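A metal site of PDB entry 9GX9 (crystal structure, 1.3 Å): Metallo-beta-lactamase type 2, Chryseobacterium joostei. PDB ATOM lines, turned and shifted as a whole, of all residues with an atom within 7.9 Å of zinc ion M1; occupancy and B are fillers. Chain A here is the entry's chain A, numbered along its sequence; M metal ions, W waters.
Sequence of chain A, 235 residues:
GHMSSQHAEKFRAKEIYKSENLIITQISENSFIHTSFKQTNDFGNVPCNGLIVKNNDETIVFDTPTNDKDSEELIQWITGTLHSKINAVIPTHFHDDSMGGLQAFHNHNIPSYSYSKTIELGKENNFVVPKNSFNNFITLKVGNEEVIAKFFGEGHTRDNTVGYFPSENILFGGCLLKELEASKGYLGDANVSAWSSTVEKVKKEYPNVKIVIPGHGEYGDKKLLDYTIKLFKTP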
ATOM      1  N   LYS A  38      -2.635 -16.823 -16.386  1.00  0.00           N
ATOM      2  CA  LYS A  38      -3.565 -15.784 -15.979  1.00  0.00           C
ATOM      3  C   LYS A  38      -4.644 -16.419 -15.122  1.00  0.00           C
ATOM      4  O   LYS A  38      -5.270 -17.407 -15.531  1.00  0.00           O
ATOM      5  CB  LYS A  38      -4.196 -15.153 -17.215  1.00  0.00           C
ATOM      6  CG  LYS A  38      -5.255 -14.101 -16.947  1.00  0.00           C
ATOM      7  CD  LYS A  38      -5.628 -13.390 -18.244  1.00  0.00           C
ATOM      8  CE  LYS A  38      -7.099 -12.966 -18.252  1.00  0.00           C
ATOM      9  NZ  LYS A  38      -7.266 -11.483 -18.292  1.00  0.00           N
ATOM     10  N   HIS A  93       0.040  -6.269 -27.033  1.00  0.00           N
ATOM     11  CA  HIS A  93      -1.206  -5.538 -26.888  1.00  0.00           C
ATOM     12  C   HIS A  93      -1.378  -5.144 -25.421  1.00  0.00           C
ATOM     13  O   HIS A  93      -0.571  -5.531 -24.577  1.00  0.00           O
ATOM     14  CB  HIS A  93      -2.401  -6.272 -27.504  1.00  0.00           C
ATOM     15  CG  HIS A  93      -2.921  -7.438 -26.733  1.00  0.00           C
ATOM     16  ND1 HIS A  93      -2.141  -8.506 -26.315  1.00  0.00           N
ATOM     17  CD2 HIS A  93      -4.187  -7.760 -26.387  1.00  0.00           C
ATOM     18  CE1 HIS A  93      -2.901  -9.408 -25.739  1.00  0.00           C
ATOM     19  NE2 HIS A  93      -4.135  -8.985 -25.762  1.00  0.00           N
ATOM     20  N   PHE A  94      -2.427  -4.367 -25.133  1.00  0.00           N
ATOM     21  CA  PHE A  94      -2.552  -3.733 -23.843  1.00  0.00           C
ATOM     22  C   PHE A  94      -3.141  -4.619 -22.760  1.00  0.00           C
ATOM     23  O   PHE A  94      -3.091  -4.241 -21.586  1.00  0.00           O
ATOM     24  CB  PHE A  94      -3.379  -2.443 -23.898  1.00  0.00           C
ATOM     25  CG  PHE A  94      -4.864  -2.669 -24.075  1.00  0.00           C
ATOM     26  CD1 PHE A  94      -5.402  -3.005 -25.296  1.00  0.00           C
ATOM     27  CD2 PHE A  94      -5.717  -2.542 -22.991  1.00  0.00           C
ATOM     28  CE1 PHE A  94      -6.759  -3.193 -25.448  1.00  0.00           C
ATOM     29  CE2 PHE A  94      -7.082  -2.725 -23.120  1.00  0.00           C
ATOM     30  CZ  PHE A  94      -7.605  -3.067 -24.357  1.00  0.00           C
ATOM     31  N   HIS A  95      -3.727  -5.760 -23.112  1.00  0.00           N
ATOM     32  CA  HIS A  95      -4.308  -6.637 -22.103  1.00  0.00           C
ATOM     33  C   HIS A  95      -3.240  -7.177 -21.161  1.00  0.00           C
ATOM     34  O   HIS A  95      -2.041  -7.252 -21.494  1.00  0.00           O
ATOM     35  CB  HIS A  95      -5.035  -7.810 -22.744  1.00  0.00           C
ATOM     36  CG  HIS A  95      -6.311  -7.460 -23.419  1.00  0.00           C
ATOM     37  ND1 HIS A  95      -6.932  -8.302 -24.316  1.00  0.00           N
ATOM     38  CD2 HIS A  95      -7.117  -6.378 -23.314  1.00  0.00           C
ATOM     39  CE1 HIS A  95      -8.051  -7.745 -24.739  1.00  0.00           C
ATOM     40  NE2 HIS A  95      -8.183  -6.573 -24.152  1.00  0.00           N
ATOM     41  N   ASP A  96      -3.688  -7.600 -19.968  1.00  0.00           N
ATOM     42  CA  ASP A  96      -2.744  -8.055 -18.948  1.00  0.00           C
ATOM     43  C   ASP A  96      -1.890  -9.243 -19.381  1.00  0.00           C
ATOM     44  O   ASP A  96      -0.748  -9.356 -18.923  1.00  0.00           O
ATOM     45  CB  ASP A  96      -3.440  -8.335 -17.619  1.00  0.00           C
ATOM     46  CG  ASP A  96      -4.481  -9.435 -17.690  1.00  0.00           C
ATOM     47  OD1 ASP A  96      -4.881  -9.874 -18.798  1.00  0.00           O
ATOM     48  OD2 ASP A  96      -4.903  -9.863 -16.592  1.00  0.00           O
ATOM     49  N   ASP A  97      -2.381 -10.119 -20.254  1.00  0.00           N
ATOM     50  CA  ASP A  97      -1.567 -11.258 -20.655  1.00  0.00           C
ATOM     51  C   ASP A  97      -0.489 -10.897 -21.661  1.00  0.00           C
ATOM     52  O   ASP A  97       0.247 -11.775 -22.104  1.00  0.00           O
ATOM     53  CB  ASP A  97      -2.436 -12.418 -21.147  1.00  0.00           C
ATOM     54  CG  ASP A  97      -3.336 -12.046 -22.279  1.00  0.00           C
ATOM     55  OD1 ASP A  97      -4.174 -11.132 -22.121  1.00  0.00           O
ATOM     56  OD2 ASP A  97      -3.218 -12.684 -23.357  1.00  0.00           O
ATOM     57  N   SER A  98      -0.383  -9.635 -22.040  1.00  0.00           N
ATOM     58  CA  SER A  98       0.775  -9.150 -22.778  1.00  0.00           C
ATOM     59  C   SER A  98       1.548  -8.068 -22.060  1.00  0.00           C
ATOM     60  O   SER A  98       2.711  -7.840 -22.397  1.00  0.00           O
ATOM     61  CB  SER A  98       0.371  -8.583 -24.156  1.00  0.00           C
ATOM     62  OG  SER A  98      -0.025  -9.608 -25.037  1.00  0.00           O
ATOM     63  N   HIS A 156      -7.816  -9.107 -32.712  1.00  0.00           N
ATOM     64  CA  HIS A 156      -8.137  -9.401 -31.323  1.00  0.00           C
ATOM     65  C   HIS A 156      -8.327  -8.131 -30.512  1.00  0.00           C
ATOM     66  O   HIS A 156      -9.247  -8.037 -29.690  1.00  0.00           O
ATOM     67  CB  HIS A 156      -7.004 -10.241 -30.761  1.00  0.00           C
ATOM     68  CG  HIS A 156      -7.104 -10.431 -29.295  1.00  0.00           C
ATOM     69  ND1 HIS A 156      -8.036 -11.270 -28.726  1.00  0.00           N
ATOM     70  CD2 HIS A 156      -6.418  -9.866 -28.279  1.00  0.00           C
ATOM     71  CE1 HIS A 156      -7.898 -11.230 -27.410  1.00  0.00           C
ATOM     72  NE2 HIS A 156      -6.935 -10.380 -27.122  1.00  0.00           N
ATOM     73  N   THR A 157      -7.474  -7.143 -30.743  1.00  0.00           N
ATOM     74  CA  THR A 157      -7.655  -5.785 -30.241  1.00  0.00           C
ATOM     75  C   THR A 157      -7.284  -4.834 -31.370  1.00  0.00           C
ATOM     76  O   THR A 157      -6.799  -5.238 -32.427  1.00  0.00           O
ATOM     77  CB  THR A 157      -6.801  -5.481 -29.003  1.00  0.00           C
ATOM     78  OG1 THR A 157      -5.437  -5.763 -29.323  1.00  0.00           O
ATOM     79  CG2 THR A 157      -7.249  -6.283 -27.815  1.00  0.00           C
ATOM     80  N   ASP A 159      -4.944  -2.599 -31.146  1.00  0.00           N
ATOM     81  CA  ASP A 159      -3.529  -2.279 -31.050  1.00  0.00           C
ATOM     82  C   ASP A 159      -2.608  -3.473 -31.245  1.00  0.00           C
ATOM     83  O   ASP A 159      -1.390  -3.309 -31.161  1.00  0.00           O
ATOM     84  CB  ASP A 159      -3.211  -1.683 -29.670  1.00  0.00           C
ATOM     85  CG  ASP A 159      -3.483  -2.663 -28.529  1.00  0.00           C
ATOM     86  OD1 ASP A 159      -4.478  -3.422 -28.618  1.00  0.00           O
ATOM     87  OD2 ASP A 159      -2.666  -2.744 -27.566  1.00  0.00           O
ATOM     88  N   ASN A 160      -3.152  -4.655 -31.532  1.00  0.00           N
ATOM     89  CA  ASN A 160      -2.316  -5.850 -31.495  1.00  0.00           C
ATOM     90  C   ASN A 160      -1.218  -5.827 -32.558  1.00  0.00           C
ATOM     91  O   ASN A 160      -1.470  -5.484 -33.721  1.00  0.00           O
ATOM     92  CB  ASN A 160      -3.133  -7.162 -31.553  1.00  0.00           C
ATOM     93  CG  ASN A 160      -4.178  -7.231 -32.664  1.00  0.00           C
ATOM     94  OD1 ASN A 160      -5.130  -8.008 -32.520  1.00  0.00           O
ATOM     95  ND2 ASN A 160      -3.993  -6.512 -33.775  1.00  0.00           N
ATOM     96  N   GLY A 174       1.094 -13.292 -31.025  1.00  0.00           N
ATOM     97  CA  GLY A 174       0.298 -12.745 -29.955  1.00  0.00           C
ATOM     98  C   GLY A 174      -1.143 -13.235 -30.045  1.00  0.00           C
ATOM     99  O   GLY A 174      -1.464 -14.246 -30.687  1.00  0.00           O
ATOM    100  N   CYS A 175      -2.033 -12.486 -29.400  1.00  0.00           N
ATOM    101  CA  CYS A 175      -3.424 -12.922 -29.318  1.00  0.00           C
ATOM    102  C   CYS A 175      -4.198 -12.710 -30.613  1.00  0.00           C
ATOM    103  O   CYS A 175      -5.330 -13.203 -30.744  1.00  0.00           O
ATOM    104  CB  CYS A 175      -4.066 -12.255 -28.106  1.00  0.00           C
ATOM    105  SG  CYS A 175      -3.174 -12.775 -26.594  1.00  0.00           S
ATOM    106  N   LEU A 176      -3.597 -12.059 -31.601  1.00  0.00           N
ATOM    107  CA  LEU A 176      -4.121 -12.044 -32.947  1.00  0.00           C
ATOM    108  C   LEU A 176      -4.111 -13.432 -33.572  1.00  0.00           C
ATOM    109  O   LEU A 176      -4.942 -13.719 -34.441  1.00  0.00           O
ATOM    110  CB  LEU A 176      -3.240 -11.110 -33.796  1.00  0.00           C
ATOM    111  CG  LEU A 176      -3.592 -10.942 -35.272  1.00  0.00           C
ATOM    112  CD1 LEU A 176      -4.891 -10.143 -35.410  1.00  0.00           C
ATOM    113  CD2 LEU A 176      -2.463 -10.240 -36.010  1.00  0.00           C
ATOM    114  N   LYS A 178      -4.463 -17.599 -33.237  1.00  0.00           N
ATOM    115  CA  LYS A 178      -5.090 -18.670 -32.473  1.00  0.00           C
ATOM    116  C   LYS A 178      -4.371 -19.977 -32.735  1.00  0.00           C
ATOM    117  O   LYS A 178      -3.860 -20.242 -33.830  1.00  0.00           O
ATOM    118  CB  LYS A 178      -6.553 -18.821 -32.863  1.00  0.00           C
ATOM    119  CG  LYS A 178      -7.438 -17.602 -32.545  1.00  0.00           C
ATOM    120  CD  LYS A 178      -7.504 -17.280 -31.081  1.00  0.00           C
ATOM    121  CE  LYS A 178      -8.512 -16.200 -30.787  1.00  0.00           C
ATOM    122  NZ  LYS A 178      -8.534 -15.916 -29.330  1.00  0.00           N
ATOM    123  N   TYR A 186     -11.893 -14.226 -26.237  1.00  0.00           N
ATOM    124  CA  TYR A 186     -12.485 -12.994 -25.749  1.00  0.00           C
ATOM    125  C   TYR A 186     -12.558 -11.963 -26.863  1.00  0.00           C
ATOM    126  O   TYR A 186     -11.530 -11.580 -27.444  1.00  0.00           O
ATOM    127  CB  TYR A 186     -11.659 -12.441 -24.602  1.00  0.00           C
ATOM    128  CG  TYR A 186     -12.134 -11.103 -24.106  1.00  0.00           C
ATOM    129  CD1 TYR A 186     -13.271 -10.985 -23.298  1.00  0.00           C
ATOM    130  CD2 TYR A 186     -11.449  -9.940 -24.438  1.00  0.00           C
ATOM    131  CE1 TYR A 186     -13.699  -9.760 -22.840  1.00  0.00           C
ATOM    132  CE2 TYR A 186     -11.877  -8.716 -23.980  1.00  0.00           C
ATOM    133  CZ  TYR A 186     -12.994  -8.633 -23.183  1.00  0.00           C
ATOM    134  OH  TYR A 186     -13.401  -7.407 -22.745  1.00  0.00           O
ATOM    135  N   ASP A 189     -12.952  -6.565 -26.939  1.00  0.00           N
ATOM    136  CA  ASP A 189     -12.176  -5.461 -27.477  1.00  0.00           C
ATOM    137  C   ASP A 189     -11.814  -5.689 -28.950  1.00  0.00           C
ATOM    138  O   ASP A 189     -10.963  -4.983 -29.498  1.00  0.00           O
ATOM    139  CB  ASP A 189     -10.896  -5.266 -26.658  1.00  0.00           C
ATOM    140  CG  ASP A 189     -11.174  -4.750 -25.248  1.00  0.00           C
ATOM    141  OD1 ASP A 189     -12.063  -3.887 -25.107  1.00  0.00           O
ATOM    142  OD2 ASP A 189     -10.478  -5.185 -24.297  1.00  0.00           O
ATOM    143  N   HIS A 216      -2.168 -17.802 -26.809  1.00  0.00           N
ATOM    144  CA  HIS A 216      -2.567 -18.854 -25.882  1.00  0.00           C
ATOM    145  C   HIS A 216      -2.490 -20.191 -26.600  1.00  0.00           C
ATOM    146  O   HIS A 216      -2.982 -20.335 -27.730  1.00  0.00           O
ATOM    147  CB  HIS A 216      -3.988 -18.636 -25.355  1.00  0.00           C
ATOM    148  CG  HIS A 216      -4.176 -17.300 -24.727  1.00  0.00           C
ATOM    149  ND1 HIS A 216      -3.733 -17.014 -23.454  1.00  0.00           N
ATOM    150  CD2 HIS A 216      -4.686 -16.151 -25.215  1.00  0.00           C
ATOM    151  CE1 HIS A 216      -3.990 -15.744 -23.174  1.00  0.00           C
ATOM    152  NE2 HIS A 216      -4.566 -15.197 -24.230  1.00  0.00           N
HETATM  153 ZN    ZN M   1      -5.963  -9.968 -25.282  1.00  0.00          ZN
HETATM  154 ZN    ZN M   2      -4.670 -13.119 -25.070  1.00  0.00          ZN
HETATM  155  O   HOH W   1      -5.683 -11.546 -24.260  1.00  0.00           O
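Asp 97 touches zinc ion M1 (OD1 to ZN, 3.8 Å).
Four residues have an atom within 4 Å of zinc ion M1: His 93, His 95, Asp 97 and His 156.
The nearest printed residue that does not touch zinc ion M1 is Cys 175 (4.1 Å).
A ring nitrogen (NE2) of His 95 sits at hydrogen-bond distance from the side-chain carboxylate (OD2) of Asp 189 (2.7 Å).
The side-chain hydroxyl (OG) of Ser 98 is in hydrogen-bond range of a ring nitrogen (ND1) of His 93, at 2.7 Å.
OD1 of Asn 160 is in hydrogen-bond range of N of His 156 (2.9 Å).
Zinc ion M1 is bound by water W1 (1.9 Å), NE2 of His 156 (2.1 Å), NE2 of His 93 (2.1 Å) and ND1 of His 95 (2.2 Å).
Zinc ion M1 has four donor atoms within binding distance.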
